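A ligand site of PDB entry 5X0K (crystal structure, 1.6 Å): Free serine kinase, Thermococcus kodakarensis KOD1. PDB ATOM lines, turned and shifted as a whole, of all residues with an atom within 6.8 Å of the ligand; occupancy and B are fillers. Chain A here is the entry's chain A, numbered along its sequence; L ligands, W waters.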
ATOM      1  N   GLU A  36       4.145  -9.436 -28.619  1.00  0.00           N
ATOM      2  CA  GLU A  36       4.925  -9.038 -27.456  1.00  0.00           C
ATOM      3  C   GLU A  36       4.278  -7.862 -26.742  1.00  0.00           C
ATOM      4  O   GLU A  36       4.239  -7.819 -25.546  1.00  0.00           O
ATOM      5  CB  GLU A  36       6.368  -8.715 -27.828  1.00  0.00           C
ATOM      6  CG  GLU A  36       7.094  -9.929 -28.364  1.00  0.00           C
ATOM      7  CD  GLU A  36       8.549  -9.656 -28.697  1.00  0.00           C
ATOM      8  OE1 GLU A  36       9.202  -8.865 -27.991  1.00  0.00           O
ATOM      9  OE2 GLU A  36       9.021 -10.271 -29.677  1.00  0.00           O
ATOM     10  N   LEU A  37       3.767  -6.904 -27.517  1.00  0.00           N
ATOM     11  CA  LEU A  37       2.985  -5.795 -26.986  1.00  0.00           C
ATOM     12  C   LEU A  37       1.798  -6.305 -26.173  1.00  0.00           C
ATOM     13  O   LEU A  37       1.556  -5.869 -25.050  1.00  0.00           O
ATOM     14  CB  LEU A  37       2.453  -4.938 -28.160  1.00  0.00           C
ATOM     15  CG  LEU A  37       1.710  -3.693 -27.672  1.00  0.00           C
ATOM     16  N   ALA A  39       1.160  -9.341 -24.840  1.00  0.00           N
ATOM     17  CA  ALA A  39       1.593 -10.047 -23.641  1.00  0.00           C
ATOM     18  C   ALA A  39       1.981  -9.120 -22.505  1.00  0.00           C
ATOM     19  O   ALA A  39       1.622  -9.353 -21.366  1.00  0.00           O
ATOM     20  CB  ALA A  39       2.702 -11.041 -23.956  1.00  0.00           C
ATOM     21  N   PHE A  40       2.732  -8.053 -22.831  1.00  0.00           N
ATOM     22  CA  PHE A  40       3.023  -7.060 -21.807  1.00  0.00           C
ATOM     23  C   PHE A  40       1.744  -6.424 -21.247  1.00  0.00           C
ATOM     24  O   PHE A  40       1.588  -6.321 -20.022  1.00  0.00           O
ATOM     25  CB  PHE A  40       4.001  -5.988 -22.283  1.00  0.00           C
ATOM     26  CG  PHE A  40       4.040  -4.852 -21.344  1.00  0.00           C
ATOM     27  CD1 PHE A  40       4.678  -4.983 -20.100  1.00  0.00           C
ATOM     28  CD2 PHE A  40       3.345  -3.684 -21.623  1.00  0.00           C
ATOM     29  CE1 PHE A  40       4.645  -3.978 -19.189  1.00  0.00           C
ATOM     30  CE2 PHE A  40       3.295  -2.662 -20.707  1.00  0.00           C
ATOM     31  CZ  PHE A  40       3.956  -2.791 -19.499  1.00  0.00           C
ATOM     32  N   SER A  43      -0.022  -8.780 -18.906  1.00  0.00           N
ATOM     33  CA  SER A  43       0.732  -8.982 -17.700  1.00  0.00           C
ATOM     34  C   SER A  43       0.627  -7.806 -16.748  1.00  0.00           C
ATOM     35  O   SER A  43       0.353  -8.000 -15.570  1.00  0.00           O
ATOM     36  CB  SER A  43       2.211  -9.242 -18.025  1.00  0.00           C
ATOM     37  OG  SER A  43       2.979  -9.427 -16.847  1.00  0.00           O
ATOM     38  N   VAL A  44       0.868  -6.591 -17.233  1.00  0.00           N
ATOM     39  CA  VAL A  44       0.910  -5.432 -16.347  1.00  0.00           C
ATOM     40  C   VAL A  44      -0.468  -5.103 -15.754  1.00  0.00           C
ATOM     41  O   VAL A  44      -0.580  -4.768 -14.569  1.00  0.00           O
ATOM     42  CB  VAL A  44       1.589  -4.185 -16.974  1.00  0.00           C
ATOM     43  CG1 VAL A  44       0.650  -3.472 -17.968  1.00  0.00           C
ATOM     44  CG2 VAL A  44       2.029  -3.224 -15.890  1.00  0.00           C
ATOM     45  N   THR A  45      -1.485  -5.232 -16.585  1.00  0.00           N
ATOM     46  CA  THR A  45      -2.852  -5.003 -16.106  1.00  0.00           C
ATOM     47  C   THR A  45      -3.274  -6.118 -15.188  1.00  0.00           C
ATOM     48  O   THR A  45      -4.117  -5.896 -14.300  1.00  0.00           O
ATOM     49  CB  THR A  45      -3.878  -4.838 -17.242  1.00  0.00           C
ATOM     50  OG1 THR A  45      -3.931  -6.003 -18.100  1.00  0.00           O
ATOM     51  CG2 THR A  45      -3.591  -3.623 -18.088  1.00  0.00           C
ATOM     52  N   SER A  47      -1.375  -7.820 -12.902  1.00  0.00           N
ATOM     53  CA  SER A  47      -0.824  -7.666 -11.548  1.00  0.00           C
ATOM     54  C   SER A  47      -0.971  -6.243 -11.020  1.00  0.00           C
ATOM     55  O   SER A  47      -1.014  -6.025  -9.819  1.00  0.00           O
ATOM     56  CB  SER A  47       0.639  -8.113 -11.510  1.00  0.00           C
ATOM     57  OG  SER A  47       1.452  -7.226 -12.250  1.00  0.00           O
ATOM     58  N   GLY A  48      -0.978  -5.271 -11.919  1.00  0.00           N
ATOM     59  CA  GLY A  48      -0.879  -3.874 -11.544  1.00  0.00           C
ATOM     60  C   GLY A  48       0.440  -3.466 -10.951  1.00  0.00           C
ATOM     61  O   GLY A  48       0.485  -2.445 -10.290  1.00  0.00           O
ATOM     62  N   ILE A  49       1.517  -4.240 -11.209  1.00  0.00           N
ATOM     63  CA  ILE A  49       2.877  -3.911 -10.764  1.00  0.00           C
ATOM     64  C   ILE A  49       3.719  -3.852 -12.007  1.00  0.00           C
ATOM     65  O   ILE A  49       3.637  -4.732 -12.875  1.00  0.00           O
ATOM     66  CB  ILE A  49       3.476  -4.966  -9.815  1.00  0.00           C
ATOM     67  CG1 ILE A  49       2.600  -5.087  -8.545  1.00  0.00           C
ATOM     68  CG2 ILE A  49       4.937  -4.666  -9.530  1.00  0.00           C
ATOM     69  CD1 ILE A  49       2.562  -3.861  -7.673  1.00  0.00           C
ATOM     70  N   PHE A  50       4.528  -2.793 -12.111  1.00  0.00           N
ATOM     71  CA  PHE A  50       5.487  -2.636 -13.178  1.00  0.00           C
ATOM     72  C   PHE A  50       6.841  -2.854 -12.525  1.00  0.00           C
ATOM     73  O   PHE A  50       7.302  -2.015 -11.777  1.00  0.00           O
ATOM     74  CB  PHE A  50       5.385  -1.236 -13.836  1.00  0.00           C
ATOM     75  CG  PHE A  50       6.250  -1.067 -15.072  1.00  0.00           C
ATOM     76  CD1 PHE A  50       7.603  -0.727 -14.940  1.00  0.00           C
ATOM     77  CD2 PHE A  50       5.743  -1.220 -16.343  1.00  0.00           C
ATOM     78  CE1 PHE A  50       8.385  -0.536 -16.085  1.00  0.00           C
ATOM     79  CE2 PHE A  50       6.520  -1.059 -17.476  1.00  0.00           C
ATOM     80  CZ  PHE A  50       7.852  -0.711 -17.340  1.00  0.00           C
ATOM     81  N   TRP A  51       7.469  -3.990 -12.792  1.00  0.00           N
ATOM     82  CA  TRP A  51       8.631  -4.444 -12.022  1.00  0.00           C
ATOM     83  C   TRP A  51       9.976  -4.418 -12.744  1.00  0.00           C
ATOM     84  O   TRP A  51      11.007  -4.780 -12.128  1.00  0.00           O
ATOM     85  CB  TRP A  51       8.352  -5.841 -11.448  1.00  0.00           C
ATOM     86  CG  TRP A  51       7.846  -6.798 -12.415  1.00  0.00           C
ATOM     87  CD1 TRP A  51       6.561  -7.232 -12.532  1.00  0.00           C
ATOM     88  CD2 TRP A  51       8.601  -7.492 -13.400  1.00  0.00           C
ATOM     89  NE1 TRP A  51       6.454  -8.119 -13.561  1.00  0.00           N
ATOM     90  CE2 TRP A  51       7.693  -8.303 -14.117  1.00  0.00           C
ATOM     91  CE3 TRP A  51       9.957  -7.512 -13.755  1.00  0.00           C
ATOM     92  CZ2 TRP A  51       8.081  -9.108 -15.174  1.00  0.00           C
ATOM     93  CZ3 TRP A  51      10.368  -8.361 -14.802  1.00  0.00           C
ATOM     94  CH2 TRP A  51       9.419  -9.132 -15.511  1.00  0.00           C
ATOM     95  N   LYS A  52      10.002  -4.028 -14.021  1.00  0.00           N
ATOM     96  CA  LYS A  52      11.185  -4.147 -14.875  1.00  0.00           C
ATOM     97  C   LYS A  52      11.476  -2.786 -15.546  1.00  0.00           C
ATOM     98  O   LYS A  52      10.848  -2.447 -16.546  1.00  0.00           O
ATOM     99  CB  LYS A  52      10.975  -5.195 -15.988  1.00  0.00           C
ATOM    100  CG  LYS A  52      12.249  -5.651 -16.689  1.00  0.00           C
ATOM    101  CD  LYS A  52      11.908  -6.598 -17.822  1.00  0.00           C
ATOM    102  CE  LYS A  52      13.148  -7.083 -18.528  1.00  0.00           C
ATOM    103  NZ  LYS A  52      12.785  -8.246 -19.360  1.00  0.00           N
ATOM    104  N   PRO A  53      12.415  -1.973 -15.018  1.00  0.00           N
ATOM    105  CA  PRO A  53      12.563  -0.617 -15.590  1.00  0.00           C
ATOM    106  C   PRO A  53      13.047  -0.627 -17.030  1.00  0.00           C
ATOM    107  O   PRO A  53      13.793  -1.528 -17.432  1.00  0.00           O
ATOM    108  CB  PRO A  53      13.633   0.043 -14.686  1.00  0.00           C
ATOM    109  CG  PRO A  53      14.383  -1.100 -14.127  1.00  0.00           C
ATOM    110  CD  PRO A  53      13.401  -2.228 -13.957  1.00  0.00           C
ATOM    111  N   MET A  54      12.621   0.381 -17.787  1.00  0.00           N
ATOM    112  CA  MET A  54      13.160   0.703 -19.106  1.00  0.00           C
ATOM    113  C   MET A  54      14.668   0.932 -18.979  1.00  0.00           C
ATOM    114  O   MET A  54      15.131   1.382 -17.929  1.00  0.00           O
ATOM    115  CB  MET A  54      12.538   1.998 -19.647  1.00  0.00           C
ATOM    116  CG  MET A  54      11.028   2.085 -19.760  1.00  0.00           C
ATOM    117  SD  MET A  54      10.475   1.038 -21.092  1.00  0.00           S
ATOM    118  CE  MET A  54      11.267   1.735 -22.566  1.00  0.00           C
ATOM    119  N   ASP A  69      16.352  -0.965 -24.099  1.00  0.00           N
ATOM    120  CA  ASP A  69      15.543  -2.171 -23.787  1.00  0.00           C
ATOM    121  C   ASP A  69      14.216  -1.677 -23.237  1.00  0.00           C
ATOM    122  O   ASP A  69      14.186  -0.836 -22.353  1.00  0.00           O
ATOM    123  CB  ASP A  69      16.290  -3.073 -22.762  1.00  0.00           C
ATOM    124  CG  ASP A  69      15.600  -4.436 -22.594  1.00  0.00           C
ATOM    125  OD1 ASP A  69      15.342  -5.106 -23.594  1.00  0.00           O
ATOM    126  OD2 ASP A  69      15.258  -4.807 -21.449  1.00  0.00           O
ATOM    127  N   GLY A  70      13.107  -2.210 -23.768  1.00  0.00           N
ATOM    128  CA  GLY A  70      11.783  -1.825 -23.322  1.00  0.00           C
ATOM    129  C   GLY A  70      10.813  -1.358 -24.387  1.00  0.00           C
ATOM    130  O   GLY A  70       9.856  -0.628 -24.023  1.00  0.00           O
ATOM    131  N   HIS A  71      11.020  -1.722 -25.639  1.00  0.00           N
ATOM    132  CA  HIS A  71      10.083  -1.281 -26.703  1.00  0.00           C
ATOM    133  C   HIS A  71       8.607  -1.622 -26.401  1.00  0.00           C
ATOM    134  O   HIS A  71       7.725  -0.789 -26.616  1.00  0.00           O
ATOM    135  CB  HIS A  71      10.457  -1.845 -28.052  1.00  0.00           C
ATOM    136  CG  HIS A  71      11.683  -1.227 -28.636  1.00  0.00           C
ATOM    137  ND1 HIS A  71      12.903  -1.852 -28.572  1.00  0.00           N
ATOM    138  CD2 HIS A  71      11.893  -0.028 -29.231  1.00  0.00           C
ATOM    139  CE1 HIS A  71      13.829  -1.073 -29.120  1.00  0.00           C
ATOM    140  NE2 HIS A  71      13.235   0.032 -29.534  1.00  0.00           N
ATOM    141  N   HIS A  72       8.329  -2.831 -25.936  1.00  0.00           N
ATOM    142  CA  HIS A  72       6.920  -3.251 -25.796  1.00  0.00           C
ATOM    143  C   HIS A  72       6.339  -2.760 -24.502  1.00  0.00           C
ATOM    144  O   HIS A  72       5.164  -2.428 -24.459  1.00  0.00           O
ATOM    145  CB  HIS A  72       6.781  -4.732 -26.039  1.00  0.00           C
ATOM    146  CG  HIS A  72       7.282  -5.133 -27.390  1.00  0.00           C
ATOM    147  ND1 HIS A  72       8.595  -5.487 -27.593  1.00  0.00           N
ATOM    148  CD2 HIS A  72       6.709  -5.128 -28.618  1.00  0.00           C
ATOM    149  CE1 HIS A  72       8.798  -5.772 -28.863  1.00  0.00           C
ATOM    150  NE2 HIS A  72       7.655  -5.558 -29.516  1.00  0.00           N
ATOM    151  N   ARG A  73       7.156  -2.647 -23.472  1.00  0.00           N
ATOM    152  CA  ARG A  73       6.747  -1.901 -22.270  1.00  0.00           C
ATOM    153  C   ARG A  73       6.315  -0.474 -22.640  1.00  0.00           C
ATOM    154  O   ARG A  73       5.235  -0.018 -22.264  1.00  0.00           O
ATOM    155  CB  ARG A  73       7.874  -1.846 -21.230  1.00  0.00           C
ATOM    156  CG  ARG A  73       7.918  -3.095 -20.372  1.00  0.00           C
ATOM    157  CD  ARG A  73       9.260  -3.255 -19.664  1.00  0.00           C
ATOM    158  NE  ARG A  73      10.264  -3.730 -20.596  1.00  0.00           N
ATOM    159  CZ  ARG A  73      11.559  -3.740 -20.325  1.00  0.00           C
ATOM    160  NH1 ARG A  73      11.975  -3.261 -19.186  1.00  0.00           N
ATOM    161  NH2 ARG A  73      12.436  -4.238 -21.203  1.00  0.00           N
ATOM    162  N   TRP A  74       7.180   0.216 -23.351  1.00  0.00           N
ATOM    163  CA  TRP A  74       6.885   1.584 -23.775  1.00  0.00           C
ATOM    164  C   TRP A  74       5.585   1.674 -24.580  1.00  0.00           C
ATOM    165  O   TRP A  74       4.681   2.470 -24.260  1.00  0.00           O
ATOM    166  CB  TRP A  74       8.051   2.136 -24.606  1.00  0.00           C
ATOM    167  CG  TRP A  74       7.785   3.423 -25.336  1.00  0.00           C
ATOM    168  CD1 TRP A  74       7.755   4.688 -24.828  1.00  0.00           C
ATOM    169  CD2 TRP A  74       7.605   3.546 -26.735  1.00  0.00           C
ATOM    170  NE1 TRP A  74       7.517   5.599 -25.841  1.00  0.00           N
ATOM    171  CE2 TRP A  74       7.461   4.933 -27.030  1.00  0.00           C
ATOM    172  CE3 TRP A  74       7.589   2.620 -27.789  1.00  0.00           C
ATOM    173  CZ2 TRP A  74       7.244   5.396 -28.331  1.00  0.00           C
ATOM    174  CZ3 TRP A  74       7.385   3.088 -29.088  1.00  0.00           C
ATOM    175  CH2 TRP A  74       7.215   4.464 -29.347  1.00  0.00           C
HETATM  176  P1  LIG L   1      10.172  -5.350 -23.999  1.00  0.00           P
HETATM  177  O1  LIG L   1       9.557  -4.187 -23.297  1.00  0.00           O
HETATM  178  O2  LIG L   1      10.368  -5.182 -25.463  1.00  0.00           O
HETATM  179  O3  LIG L   1      11.405  -5.867 -23.299  1.00  0.00           O
HETATM  180  O4  LIG L   1       9.048  -6.534 -23.932  1.00  0.00           O
HETATM  181  C1  LIG L   1       8.084  -6.568 -22.897  1.00  0.00           C
HETATM  182  C2  LIG L   1       8.749  -6.823 -21.543  1.00  0.00           C
HETATM  183  O5  LIG L   1       7.781  -6.648 -20.526  1.00  0.00           O
HETATM  184  C3  LIG L   1       9.282  -8.234 -21.346  1.00  0.00           C
HETATM  185  O6  LIG L   1      10.700  -8.184 -21.215  1.00  0.00           O
HETATM  186  C4  LIG L   1       8.636  -8.727 -20.070  1.00  0.00           C
HETATM  187  O7  LIG L   1       9.498  -9.437 -19.157  1.00  0.00           O
HETATM  188  C5  LIG L   1       8.204  -7.423 -19.437  1.00  0.00           C
HETATM  189  N1  LIG L   1       7.105  -7.485 -18.485  1.00  0.00           N
HETATM  190  C6  LIG L   1       6.113  -8.411 -18.366  1.00  0.00           C
HETATM  191  N2  LIG L   1       5.288  -8.069 -17.358  1.00  0.00           N
HETATM  192  C7  LIG L   1       5.733  -6.901 -16.848  1.00  0.00           C
HETATM  193  C8  LIG L   1       5.302  -6.044 -15.754  1.00  0.00           C
HETATM  194  N3  LIG L   1       4.211  -6.354 -15.017  1.00  0.00           N
HETATM  195  N4  LIG L   1       6.052  -4.924 -15.516  1.00  0.00           N
HETATM  196  C9  LIG L   1       7.135  -4.632 -16.295  1.00  0.00           C
HETATM  197  N5  LIG L   1       7.608  -5.389 -17.303  1.00  0.00           N
HETATM  198  C10 LIG L   1       6.932  -6.528 -17.594  1.00  0.00           C
HETATM  199  O   HOH W   1      13.069  -3.747 -26.203  1.00  0.00           O
HETATM  200  O   HOH W   2       9.027  -8.841 -25.431  1.00  0.00           O
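A ring nitrogen (ND1) of His 72 lies close to the side-chain carboxylate of Glu 36 (3.5 Å).
The backbone carbonyl oxygen of Lys 52 lies within hydrogen-bond range of the guanidinium group of Arg 73 (3.0 Å).
The backbone NH of Ile 49 is in hydrogen-bond range of the side-chain hydroxyl of Ser 47 (3.2 Å).
The backbone carbonyl oxygen of Pro 53 lies within hydrogen-bond range of the guanidinium group of Arg 73 (3.1 Å).
The guanidinium group (NH2) of Arg 73 lies within salt-bridge range of the side-chain carboxylate (OD2) of Asp 69, 2.9 Å away.
NE of Arg 73 lies within salt-bridge range of O1 of the ligand, 2.8 Å away.
N4 of the ligand sits at hydrogen-bond distance from N of Trp 51, at 3.2 Å.
O1 of the ligand lies within hydrogen-bond range of N of Arg 73.
The side-chain amino group of Lys 52 is in hydrogen-bond range of an oxygen (O6) of the ligand (2.8 Å).
OG of Ser 43 is in hydrogen-bond range of N2 of the ligand (2.7 Å).
The backbone carbonyl oxygen (O) of Ile 49 is in hydrogen-bond range of a nitrogen (N3) of the ligand, at 2.7 Å.
O2 of the ligand sits at hydrogen-bond distance from ND1 of His 72 (2.8 Å).
An oxygen (O2) of the ligand sits at hydrogen-bond distance from the backbone NH (N) of His 72 (3.1 Å).
Water W2 lies within hydrogen-bond range of OE1 of Glu 36 (2.6 Å) and O4 of the ligand (2.8 Å).
Water W1 lies within hydrogen-bond range of the backbone NH (N) of Gly 70 (2.9 Å), the backbone NH (N) of His 71 (2.9 Å) and an oxygen (O2) of the ligand (3.1 Å).
Merely in contact with the ligand: Phe 40 (3.5 Å), Val 44 (3.7 Å), Phe 50 (3.3 Å), Gly 70 (3.2 Å) and His 71 (3.5 Å).
Hydrophobic or aromatic side chains that line the ligand: Phe 40, Val 44, Phe 50, Trp 51 and His 72.
Within 4 Å of the ligand: Phe 40, Ser 43, Val 44, Ile 49, Phe 50, Trp 51, Lys 52, Gly 70, His 71, His 72 and Arg 73.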
